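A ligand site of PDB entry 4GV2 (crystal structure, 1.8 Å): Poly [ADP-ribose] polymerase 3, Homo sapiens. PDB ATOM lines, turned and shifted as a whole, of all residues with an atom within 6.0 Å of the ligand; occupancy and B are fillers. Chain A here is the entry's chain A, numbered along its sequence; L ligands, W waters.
ND1 of His 209 sits at hydrogen-bond distance from O of Tyr 239 (2.7 Å). The side-chain carboxylate (OE2) of Glu 339 is in salt-bridge range of the side-chain amino group (NZ) of Lys 246 (3.8 Å). The backbone NH (N) of Phe 240 sits at hydrogen-bond distance from the backbone carbonyl oxygen (O) of Tyr 340 (2.8 Å). OD1 of Asp 116 lies within salt-bridge range of NH1 of Arg 225 (2.8 Å). The side-chain hydroxyl of Tyr 250 sits at hydrogen-bond distance from the side-chain amino group of Lys 246 (3.1 Å). The backbone NH (N) of Met 227 lies within hydrogen-bond range of the side-chain hydroxyl (OG) of Ser 230. The side-chain hydroxyl (OG) of Ser 247 lies close to the backbone carbonyl oxygen (O) of Trp 208, 3.3 Å away.
N of Gly 210 sits at hydrogen-bond distance from O2 of the ligand (2.8 Å). The backbone carbonyl oxygen of Gly 210 lies within hydrogen-bond range of a nitrogen (N4) of the ligand, at 2.8 Å. The side-chain hydroxyl (OG) of Ser 247 is in hydrogen-bond range of an oxygen (O2) of the ligand (2.8 Å).
Water W5 bridges the side-chain hydroxyl of Ser 230 (2.7 Å) and a nitrogen (N1) of the ligand (2.8 Å). Water W4 lies within hydrogen-bond range of O1 of the ligand (2.8 Å) and N of Tyr 239 (3.1 Å). Water W3 lies within hydrogen-bond range of the backbone carbonyl oxygen (O) of Leu 112 (2.8 Å) and the side-chain carboxylate (OD1) of Asp 116 (3.1 Å).
Leu 112 touches the ligand (O to C2, 3.7 Å). Asp 116 touches the ligand (OD2 to C3, 3.1 Å). CA of His 209 touches O2 of the ligand, at 3.4 Å. Val 215 touches the ligand (CG1 to C2, 3.9 Å). Met 227 touches the ligand (SD to C4, 3.8 Å). Tyr 239 touches the ligand. O of Phe 240 touches C15 of the ligand, 3.7 Å away. Tyr 250 touches the ligand. Glu 339 touches the ligand (OE1 to C14, 3.6 Å). Hydrophobic or aromatic side chains within 4 Å of the ligand: Leu 112, His 209, Val 215, Met 227, Tyr 239 and Tyr 250. Of the 22 residues printed, 11 come within 4 Å of the ligand. Along chain A the residues within 4 Å of the ligand span positions 112 to 339.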
ATOM      1  N   ASP A 109     -12.562 -29.718  -0.423  1.00  0.00           N
ATOM      2  CA  ASP A 109     -12.715 -28.401   0.189  1.00  0.00           C
ATOM      3  C   ASP A 109     -13.262 -27.345  -0.812  1.00  0.00           C
ATOM      4  O   ASP A 109     -14.121 -26.521  -0.442  1.00  0.00           O
ATOM      5  CB  ASP A 109     -11.399 -27.952   0.795  1.00  0.00           C
ATOM      6  CG  ASP A 109     -11.047 -28.714   2.062  1.00  0.00           C
ATOM      7  OD1 ASP A 109     -11.893 -29.506   2.538  1.00  0.00           O
ATOM      8  OD2 ASP A 109      -9.917 -28.511   2.601  1.00  0.00           O
ATOM      9  N   LEU A 112     -16.915 -28.018  -1.139  1.00  0.00           N
ATOM     10  CA  LEU A 112     -17.641 -27.554   0.075  1.00  0.00           C
ATOM     11  C   LEU A 112     -17.880 -26.034   0.022  1.00  0.00           C
ATOM     12  O   LEU A 112     -18.943 -25.549   0.384  1.00  0.00           O
ATOM     13  CB  LEU A 112     -16.891 -27.921   1.337  1.00  0.00           C
ATOM     14  CG  LEU A 112     -16.927 -29.416   1.736  1.00  0.00           C
ATOM     15  CD1 LEU A 112     -15.980 -29.703   2.888  1.00  0.00           C
ATOM     16  CD2 LEU A 112     -18.302 -29.811   2.164  1.00  0.00           C
ATOM     17  N   VAL A 113     -16.897 -25.292  -0.459  1.00  0.00           N
ATOM     18  CA  VAL A 113     -17.061 -23.868  -0.661  1.00  0.00           C
ATOM     19  C   VAL A 113     -18.106 -23.636  -1.765  1.00  0.00           C
ATOM     20  O   VAL A 113     -19.032 -22.831  -1.601  1.00  0.00           O
ATOM     21  CB  VAL A 113     -15.701 -23.178  -1.037  1.00  0.00           C
ATOM     22  CG1 VAL A 113     -15.965 -21.738  -1.518  1.00  0.00           C
ATOM     23  CG2 VAL A 113     -14.738 -23.170   0.171  1.00  0.00           C
ATOM     24  N   ASP A 116     -21.619 -23.972  -0.563  1.00  0.00           N
ATOM     25  CA  ASP A 116     -22.074 -22.786   0.147  1.00  0.00           C
ATOM     26  C   ASP A 116     -22.377 -21.601  -0.753  1.00  0.00           C
ATOM     27  O   ASP A 116     -23.251 -20.785  -0.441  1.00  0.00           O
ATOM     28  CB  ASP A 116     -21.080 -22.412   1.271  1.00  0.00           C
ATOM     29  CG  ASP A 116     -21.239 -23.298   2.516  1.00  0.00           C
ATOM     30  OD1 ASP A 116     -22.237 -24.134   2.543  1.00  0.00           O
ATOM     31  OD2 ASP A 116     -20.445 -23.102   3.490  1.00  0.00           O
ATOM     32  N   TRP A 208     -11.524 -18.246  17.574  1.00  0.00           N
ATOM     33  CA  TRP A 208     -11.595 -17.715  16.205  1.00  0.00           C
ATOM     34  C   TRP A 208     -11.963 -18.798  15.189  1.00  0.00           C
ATOM     35  O   TRP A 208     -11.545 -19.973  15.313  1.00  0.00           O
ATOM     36  CB  TRP A 208     -10.243 -17.139  15.799  1.00  0.00           C
ATOM     37  CG  TRP A 208      -9.792 -15.977  16.638  1.00  0.00           C
ATOM     38  CD1 TRP A 208      -8.885 -16.005  17.661  1.00  0.00           C
ATOM     39  CD2 TRP A 208     -10.293 -14.653  16.566  1.00  0.00           C
ATOM     40  NE1 TRP A 208      -8.738 -14.720  18.197  1.00  0.00           N
ATOM     41  CE2 TRP A 208      -9.616 -13.889  17.560  1.00  0.00           C
ATOM     42  CE3 TRP A 208     -11.224 -14.016  15.757  1.00  0.00           C
ATOM     43  CZ2 TRP A 208      -9.843 -12.547  17.744  1.00  0.00           C
ATOM     44  CZ3 TRP A 208     -11.460 -12.670  15.938  1.00  0.00           C
ATOM     45  CH2 TRP A 208     -10.792 -11.937  16.950  1.00  0.00           C
ATOM     46  N   HIS A 209     -12.705 -18.380  14.156  1.00  0.00           N
ATOM     47  CA  HIS A 209     -12.929 -19.196  12.983  1.00  0.00           C
ATOM     48  C   HIS A 209     -12.874 -18.288  11.746  1.00  0.00           C
ATOM     49  O   HIS A 209     -13.708 -17.414  11.566  1.00  0.00           O
ATOM     50  CB  HIS A 209     -14.258 -19.949  13.082  1.00  0.00           C
ATOM     51  CG  HIS A 209     -14.494 -20.886  11.932  1.00  0.00           C
ATOM     52  ND1 HIS A 209     -14.010 -22.173  11.917  1.00  0.00           N
ATOM     53  CD2 HIS A 209     -15.177 -20.719  10.767  1.00  0.00           C
ATOM     54  CE1 HIS A 209     -14.385 -22.774  10.792  1.00  0.00           C
ATOM     55  NE2 HIS A 209     -15.055 -21.900  10.057  1.00  0.00           N
ATOM     56  N   GLY A 210     -11.841 -18.456  10.940  1.00  0.00           N
ATOM     57  CA  GLY A 210     -11.676 -17.665   9.703  1.00  0.00           C
ATOM     58  C   GLY A 210     -12.155 -18.428   8.504  1.00  0.00           C
ATOM     59  O   GLY A 210     -11.913 -19.631   8.426  1.00  0.00           O
ATOM     60  N   THR A 211     -12.733 -17.767   7.478  1.00  0.00           N
ATOM     61  CA  THR A 211     -13.192 -18.457   6.310  1.00  0.00           C
ATOM     62  C   THR A 211     -13.137 -17.586   5.033  1.00  0.00           C
ATOM     63  O   THR A 211     -12.931 -16.481   5.147  1.00  0.00           O
ATOM     64  CB  THR A 211     -14.686 -18.855   6.443  1.00  0.00           C
ATOM     65  OG1 THR A 211     -15.479 -17.701   6.288  1.00  0.00           O
ATOM     66  CG2 THR A 211     -14.986 -19.465   7.733  1.00  0.00           C
ATOM     67  N   VAL A 215     -18.411 -18.035   2.017  1.00  0.00           N
ATOM     68  CA  VAL A 215     -19.189 -18.938   2.844  1.00  0.00           C
ATOM     69  C   VAL A 215     -19.821 -18.235   4.054  1.00  0.00           C
ATOM     70  O   VAL A 215     -20.486 -18.888   4.868  1.00  0.00           O
ATOM     71  CB  VAL A 215     -18.397 -20.188   3.230  1.00  0.00           C
ATOM     72  CG1 VAL A 215     -17.704 -20.793   1.986  1.00  0.00           C
ATOM     73  CG2 VAL A 215     -17.381 -19.865   4.341  1.00  0.00           C
ATOM     74  N   ARG A 225     -20.753 -25.916  10.432  1.00  0.00           N
ATOM     75  CA  ARG A 225     -21.186 -27.282  10.142  1.00  0.00           C
ATOM     76  C   ARG A 225     -20.022 -28.239   9.951  1.00  0.00           C
ATOM     77  O   ARG A 225     -18.898 -27.856   9.578  1.00  0.00           O
ATOM     78  CB  ARG A 225     -22.017 -27.238   8.829  1.00  0.00           C
ATOM     79  CG  ARG A 225     -23.403 -26.591   9.014  1.00  0.00           C
ATOM     80  CD  ARG A 225     -23.867 -25.821   7.746  1.00  0.00           C
ATOM     81  NE  ARG A 225     -22.923 -24.723   7.453  1.00  0.00           N
ATOM     82  CZ  ARG A 225     -22.534 -24.306   6.237  1.00  0.00           C
ATOM     83  NH1 ARG A 225     -23.039 -24.805   5.109  1.00  0.00           N
ATOM     84  NH2 ARG A 225     -21.583 -23.395   6.138  1.00  0.00           N
ATOM     85  N   MET A 227     -19.488 -31.468   7.518  1.00  0.00           N
ATOM     86  CA  MET A 227     -20.041 -32.189   6.339  1.00  0.00           C
ATOM     87  C   MET A 227     -19.389 -33.505   6.128  1.00  0.00           C
ATOM     88  O   MET A 227     -18.252 -33.701   6.564  1.00  0.00           O
ATOM     89  CB  MET A 227     -19.829 -31.410   5.070  1.00  0.00           C
ATOM     90  CG  MET A 227     -20.766 -30.325   4.877  1.00  0.00           C
ATOM     91  SD  MET A 227     -20.351 -28.994   5.965  1.00  0.00           S
ATOM     92  CE  MET A 227     -21.938 -28.180   5.654  1.00  0.00           C
ATOM     93  N   SER A 230     -15.821 -33.103   5.042  1.00  0.00           N
ATOM     94  CA  SER A 230     -14.949 -32.226   5.856  1.00  0.00           C
ATOM     95  C   SER A 230     -13.723 -33.045   6.317  1.00  0.00           C
ATOM     96  O   SER A 230     -13.870 -34.206   6.670  1.00  0.00           O
ATOM     97  CB  SER A 230     -15.653 -31.759   7.129  1.00  0.00           C
ATOM     98  OG  SER A 230     -16.779 -30.957   6.850  1.00  0.00           O
ATOM     99  N   TYR A 239     -13.174 -26.629  13.154  1.00  0.00           N
ATOM    100  CA  TYR A 239     -11.841 -26.162  13.525  1.00  0.00           C
ATOM    101  C   TYR A 239     -11.896 -24.734  14.019  1.00  0.00           C
ATOM    102  O   TYR A 239     -12.543 -23.877  13.395  1.00  0.00           O
ATOM    103  CB  TYR A 239     -10.908 -26.202  12.301  1.00  0.00           C
ATOM    104  CG  TYR A 239     -10.489 -27.599  11.909  1.00  0.00           C
ATOM    105  CD1 TYR A 239      -9.210 -28.046  12.203  1.00  0.00           C
ATOM    106  CD2 TYR A 239     -11.363 -28.454  11.258  1.00  0.00           C
ATOM    107  CE1 TYR A 239      -8.830 -29.281  11.853  1.00  0.00           C
ATOM    108  CE2 TYR A 239     -10.940 -29.745  10.892  1.00  0.00           C
ATOM    109  CZ  TYR A 239      -9.679 -30.145  11.222  1.00  0.00           C
ATOM    110  OH  TYR A 239      -9.218 -31.414  10.895  1.00  0.00           O
ATOM    111  N   PHE A 240     -11.255 -24.494  15.156  1.00  0.00           N
ATOM    112  CA  PHE A 240     -11.082 -23.170  15.674  1.00  0.00           C
ATOM    113  C   PHE A 240      -9.655 -22.921  16.135  1.00  0.00           C
ATOM    114  O   PHE A 240      -8.840 -23.843  16.284  1.00  0.00           O
ATOM    115  CB  PHE A 240     -11.960 -22.954  16.920  1.00  0.00           C
ATOM    116  CG  PHE A 240     -13.386 -23.171  16.724  1.00  0.00           C
ATOM    117  CD1 PHE A 240     -14.235 -22.084  16.453  1.00  0.00           C
ATOM    118  CD2 PHE A 240     -13.943 -24.464  16.790  1.00  0.00           C
ATOM    119  CE1 PHE A 240     -15.580 -22.282  16.256  1.00  0.00           C
ATOM    120  CE2 PHE A 240     -15.304 -24.636  16.621  1.00  0.00           C
ATOM    121  CZ  PHE A 240     -16.122 -23.531  16.361  1.00  0.00           C
ATOM    122  N   ALA A 241      -9.314 -21.665  16.321  1.00  0.00           N
ATOM    123  CA  ALA A 241      -7.987 -21.307  16.867  1.00  0.00           C
ATOM    124  C   ALA A 241      -8.126 -20.317  18.008  1.00  0.00           C
ATOM    125  O   ALA A 241      -9.036 -19.465  18.009  1.00  0.00           O
ATOM    126  CB  ALA A 241      -7.078 -20.721  15.792  1.00  0.00           C
ATOM    127  N   LYS A 246      -3.567 -17.678  13.357  1.00  0.00           N
ATOM    128  CA  LYS A 246      -3.825 -18.985  12.746  1.00  0.00           C
ATOM    129  C   LYS A 246      -5.113 -18.968  11.897  1.00  0.00           C
ATOM    130  O   LYS A 246      -5.113 -19.328  10.711  1.00  0.00           O
ATOM    131  CB  LYS A 246      -3.898 -20.074  13.846  1.00  0.00           C
ATOM    132  CG  LYS A 246      -4.357 -21.408  13.343  1.00  0.00           C
ATOM    133  CD  LYS A 246      -3.266 -21.978  12.409  1.00  0.00           C
ATOM    134  CE  LYS A 246      -3.725 -23.253  11.694  1.00  0.00           C
ATOM    135  NZ  LYS A 246      -2.690 -23.653  10.643  1.00  0.00           N
ATOM    136  N   SER A 247      -6.203 -18.467  12.467  1.00  0.00           N
ATOM    137  CA  SER A 247      -7.456 -18.349  11.752  1.00  0.00           C
ATOM    138  C   SER A 247      -7.370 -17.372  10.584  1.00  0.00           C
ATOM    139  O   SER A 247      -8.040 -17.573   9.559  1.00  0.00           O
ATOM    140  CB  SER A 247      -8.588 -17.939  12.690  1.00  0.00           C
ATOM    141  OG  SER A 247      -8.955 -19.049  13.511  1.00  0.00           O
ATOM    142  N   ALA A 248      -6.586 -16.312  10.748  1.00  0.00           N
ATOM    143  CA  ALA A 248      -6.492 -15.285   9.713  1.00  0.00           C
ATOM    144  C   ALA A 248      -5.925 -15.850   8.404  1.00  0.00           C
ATOM    145  O   ALA A 248      -6.221 -15.327   7.342  1.00  0.00           O
ATOM    146  CB  ALA A 248      -5.626 -14.137  10.181  1.00  0.00           C
ATOM    147  N   TYR A 250      -6.858 -18.415   6.948  1.00  0.00           N
ATOM    148  CA  TYR A 250      -7.940 -19.024   6.214  1.00  0.00           C
ATOM    149  C   TYR A 250      -8.910 -17.981   5.712  1.00  0.00           C
ATOM    150  O   TYR A 250      -9.871 -18.303   5.020  1.00  0.00           O
ATOM    151  CB  TYR A 250      -8.662 -20.090   7.067  1.00  0.00           C
ATOM    152  CG  TYR A 250      -7.745 -21.175   7.549  1.00  0.00           C
ATOM    153  CD1 TYR A 250      -7.495 -22.300   6.770  1.00  0.00           C
ATOM    154  CD2 TYR A 250      -7.111 -21.073   8.752  1.00  0.00           C
ATOM    155  CE1 TYR A 250      -6.638 -23.316   7.219  1.00  0.00           C
ATOM    156  CE2 TYR A 250      -6.252 -22.064   9.201  1.00  0.00           C
ATOM    157  CZ  TYR A 250      -6.020 -23.179   8.418  1.00  0.00           C
ATOM    158  OH  TYR A 250      -5.145 -24.135   8.879  1.00  0.00           O
ATOM    159  N   SER A 338      -2.230 -23.934  18.126  1.00  0.00           N
ATOM    160  CA  SER A 338      -3.274 -24.886  18.484  1.00  0.00           C
ATOM    161  C   SER A 338      -4.457 -24.857  17.511  1.00  0.00           C
ATOM    162  O   SER A 338      -4.844 -23.810  16.999  1.00  0.00           O
ATOM    163  CB  SER A 338      -3.783 -24.634  19.919  1.00  0.00           C
ATOM    164  OG  SER A 338      -2.744 -24.810  20.878  1.00  0.00           O
ATOM    165  N   GLU A 339      -5.035 -26.033  17.286  1.00  0.00           N
ATOM    166  CA  GLU A 339      -6.307 -26.216  16.605  1.00  0.00           C
ATOM    167  C   GLU A 339      -7.270 -26.881  17.583  1.00  0.00           C
ATOM    168  O   GLU A 339      -6.968 -27.958  18.138  1.00  0.00           O
ATOM    169  CB  GLU A 339      -6.113 -27.080  15.368  1.00  0.00           C
ATOM    170  CG  GLU A 339      -4.963 -26.569  14.480  1.00  0.00           C
ATOM    171  CD  GLU A 339      -4.908 -27.160  13.073  1.00  0.00           C
ATOM    172  OE1 GLU A 339      -5.815 -27.887  12.655  1.00  0.00           O
ATOM    173  OE2 GLU A 339      -3.923 -26.854  12.374  1.00  0.00           O
ATOM    174  N   TYR A 340      -8.401 -26.217  17.802  1.00  0.00           N
ATOM    175  CA  TYR A 340      -9.435 -26.624  18.731  1.00  0.00           C
ATOM    176  C   TYR A 340     -10.573 -27.279  17.926  1.00  0.00           C
ATOM    177  O   TYR A 340     -11.121 -26.652  16.995  1.00  0.00           O
ATOM    178  CB  TYR A 340      -9.962 -25.429  19.471  1.00  0.00           C
ATOM    179  CG  TYR A 340      -9.066 -24.857  20.577  1.00  0.00           C
ATOM    180  CD1 TYR A 340      -9.431 -24.980  21.924  1.00  0.00           C
ATOM    181  CD2 TYR A 340      -7.893 -24.175  20.290  1.00  0.00           C
ATOM    182  CE1 TYR A 340      -8.671 -24.454  22.911  1.00  0.00           C
ATOM    183  CE2 TYR A 340      -7.119 -23.633  21.302  1.00  0.00           C
ATOM    184  CZ  TYR A 340      -7.506 -23.812  22.613  1.00  0.00           C
ATOM    185  OH  TYR A 340      -6.751 -23.257  23.635  1.00  0.00           O
HETATM  186  C1  LIG L   1     -16.097 -24.469   3.899  1.00  0.00           C
HETATM  187  C2  LIG L   1     -17.459 -24.393   3.554  1.00  0.00           C
HETATM  188  C3  LIG L   1     -18.328 -25.355   4.038  1.00  0.00           C
HETATM  189  C4  LIG L   1     -17.834 -26.373   4.853  1.00  0.00           C
HETATM  190  N1  LIG L   1     -16.452 -26.450   5.206  1.00  0.00           N
HETATM  191  C5  LIG L   1     -15.637 -25.488   4.756  1.00  0.00           C
HETATM  192  C6  LIG L   1     -14.318 -25.622   5.102  1.00  0.00           C
HETATM  193  C7  LIG L   1     -13.557 -25.828   3.734  1.00  0.00           C
HETATM  194  N2  LIG L   1     -13.617 -24.515   5.736  1.00  0.00           N
HETATM  195  C8  LIG L   1     -12.933 -24.498   6.924  1.00  0.00           C
HETATM  196  O1  LIG L   1     -12.959 -25.256   7.885  1.00  0.00           O
HETATM  197  C9  LIG L   1     -11.974 -23.346   6.794  1.00  0.00           C
HETATM  198  C10 LIG L   1     -11.230 -22.590   7.781  1.00  0.00           C
HETATM  199  C11 LIG L   1     -10.575 -22.833   8.946  1.00  0.00           C
HETATM  200  N3  LIG L   1      -9.726 -23.838   9.205  1.00  0.00           N
HETATM  201  C12 LIG L   1      -9.067 -23.819  10.406  1.00  0.00           C
HETATM  202  C13 LIG L   1      -8.186 -24.875  10.706  1.00  0.00           C
HETATM  203  C14 LIG L   1      -7.490 -24.842  11.882  1.00  0.00           C
HETATM  204  C15 LIG L   1      -7.632 -23.805  12.793  1.00  0.00           C
HETATM  205  C16 LIG L   1      -8.478 -22.723  12.449  1.00  0.00           C
HETATM  206  C17 LIG L   1      -9.179 -22.743  11.276  1.00  0.00           C
HETATM  207  C18 LIG L   1     -10.030 -21.690  10.941  1.00  0.00           C
HETATM  208  O2  LIG L   1     -10.180 -20.667  11.603  1.00  0.00           O
HETATM  209  N4  LIG L   1     -10.675 -21.767   9.745  1.00  0.00           N
HETATM  210  O   HOH W   1     -12.066 -27.898   7.516  1.00  0.00           O
HETATM  211  O   HOH W   2      -9.940 -26.037   7.238  1.00  0.00           O
HETATM  212  O   HOH W   3     -20.665 -26.820   2.140  1.00  0.00           O
HETATM  213  O   HOH W   4     -14.193 -26.122  10.219  1.00  0.00           O
HETATM  214  O   HOH W   5     -15.570 -28.490   6.830  1.00  0.00           O
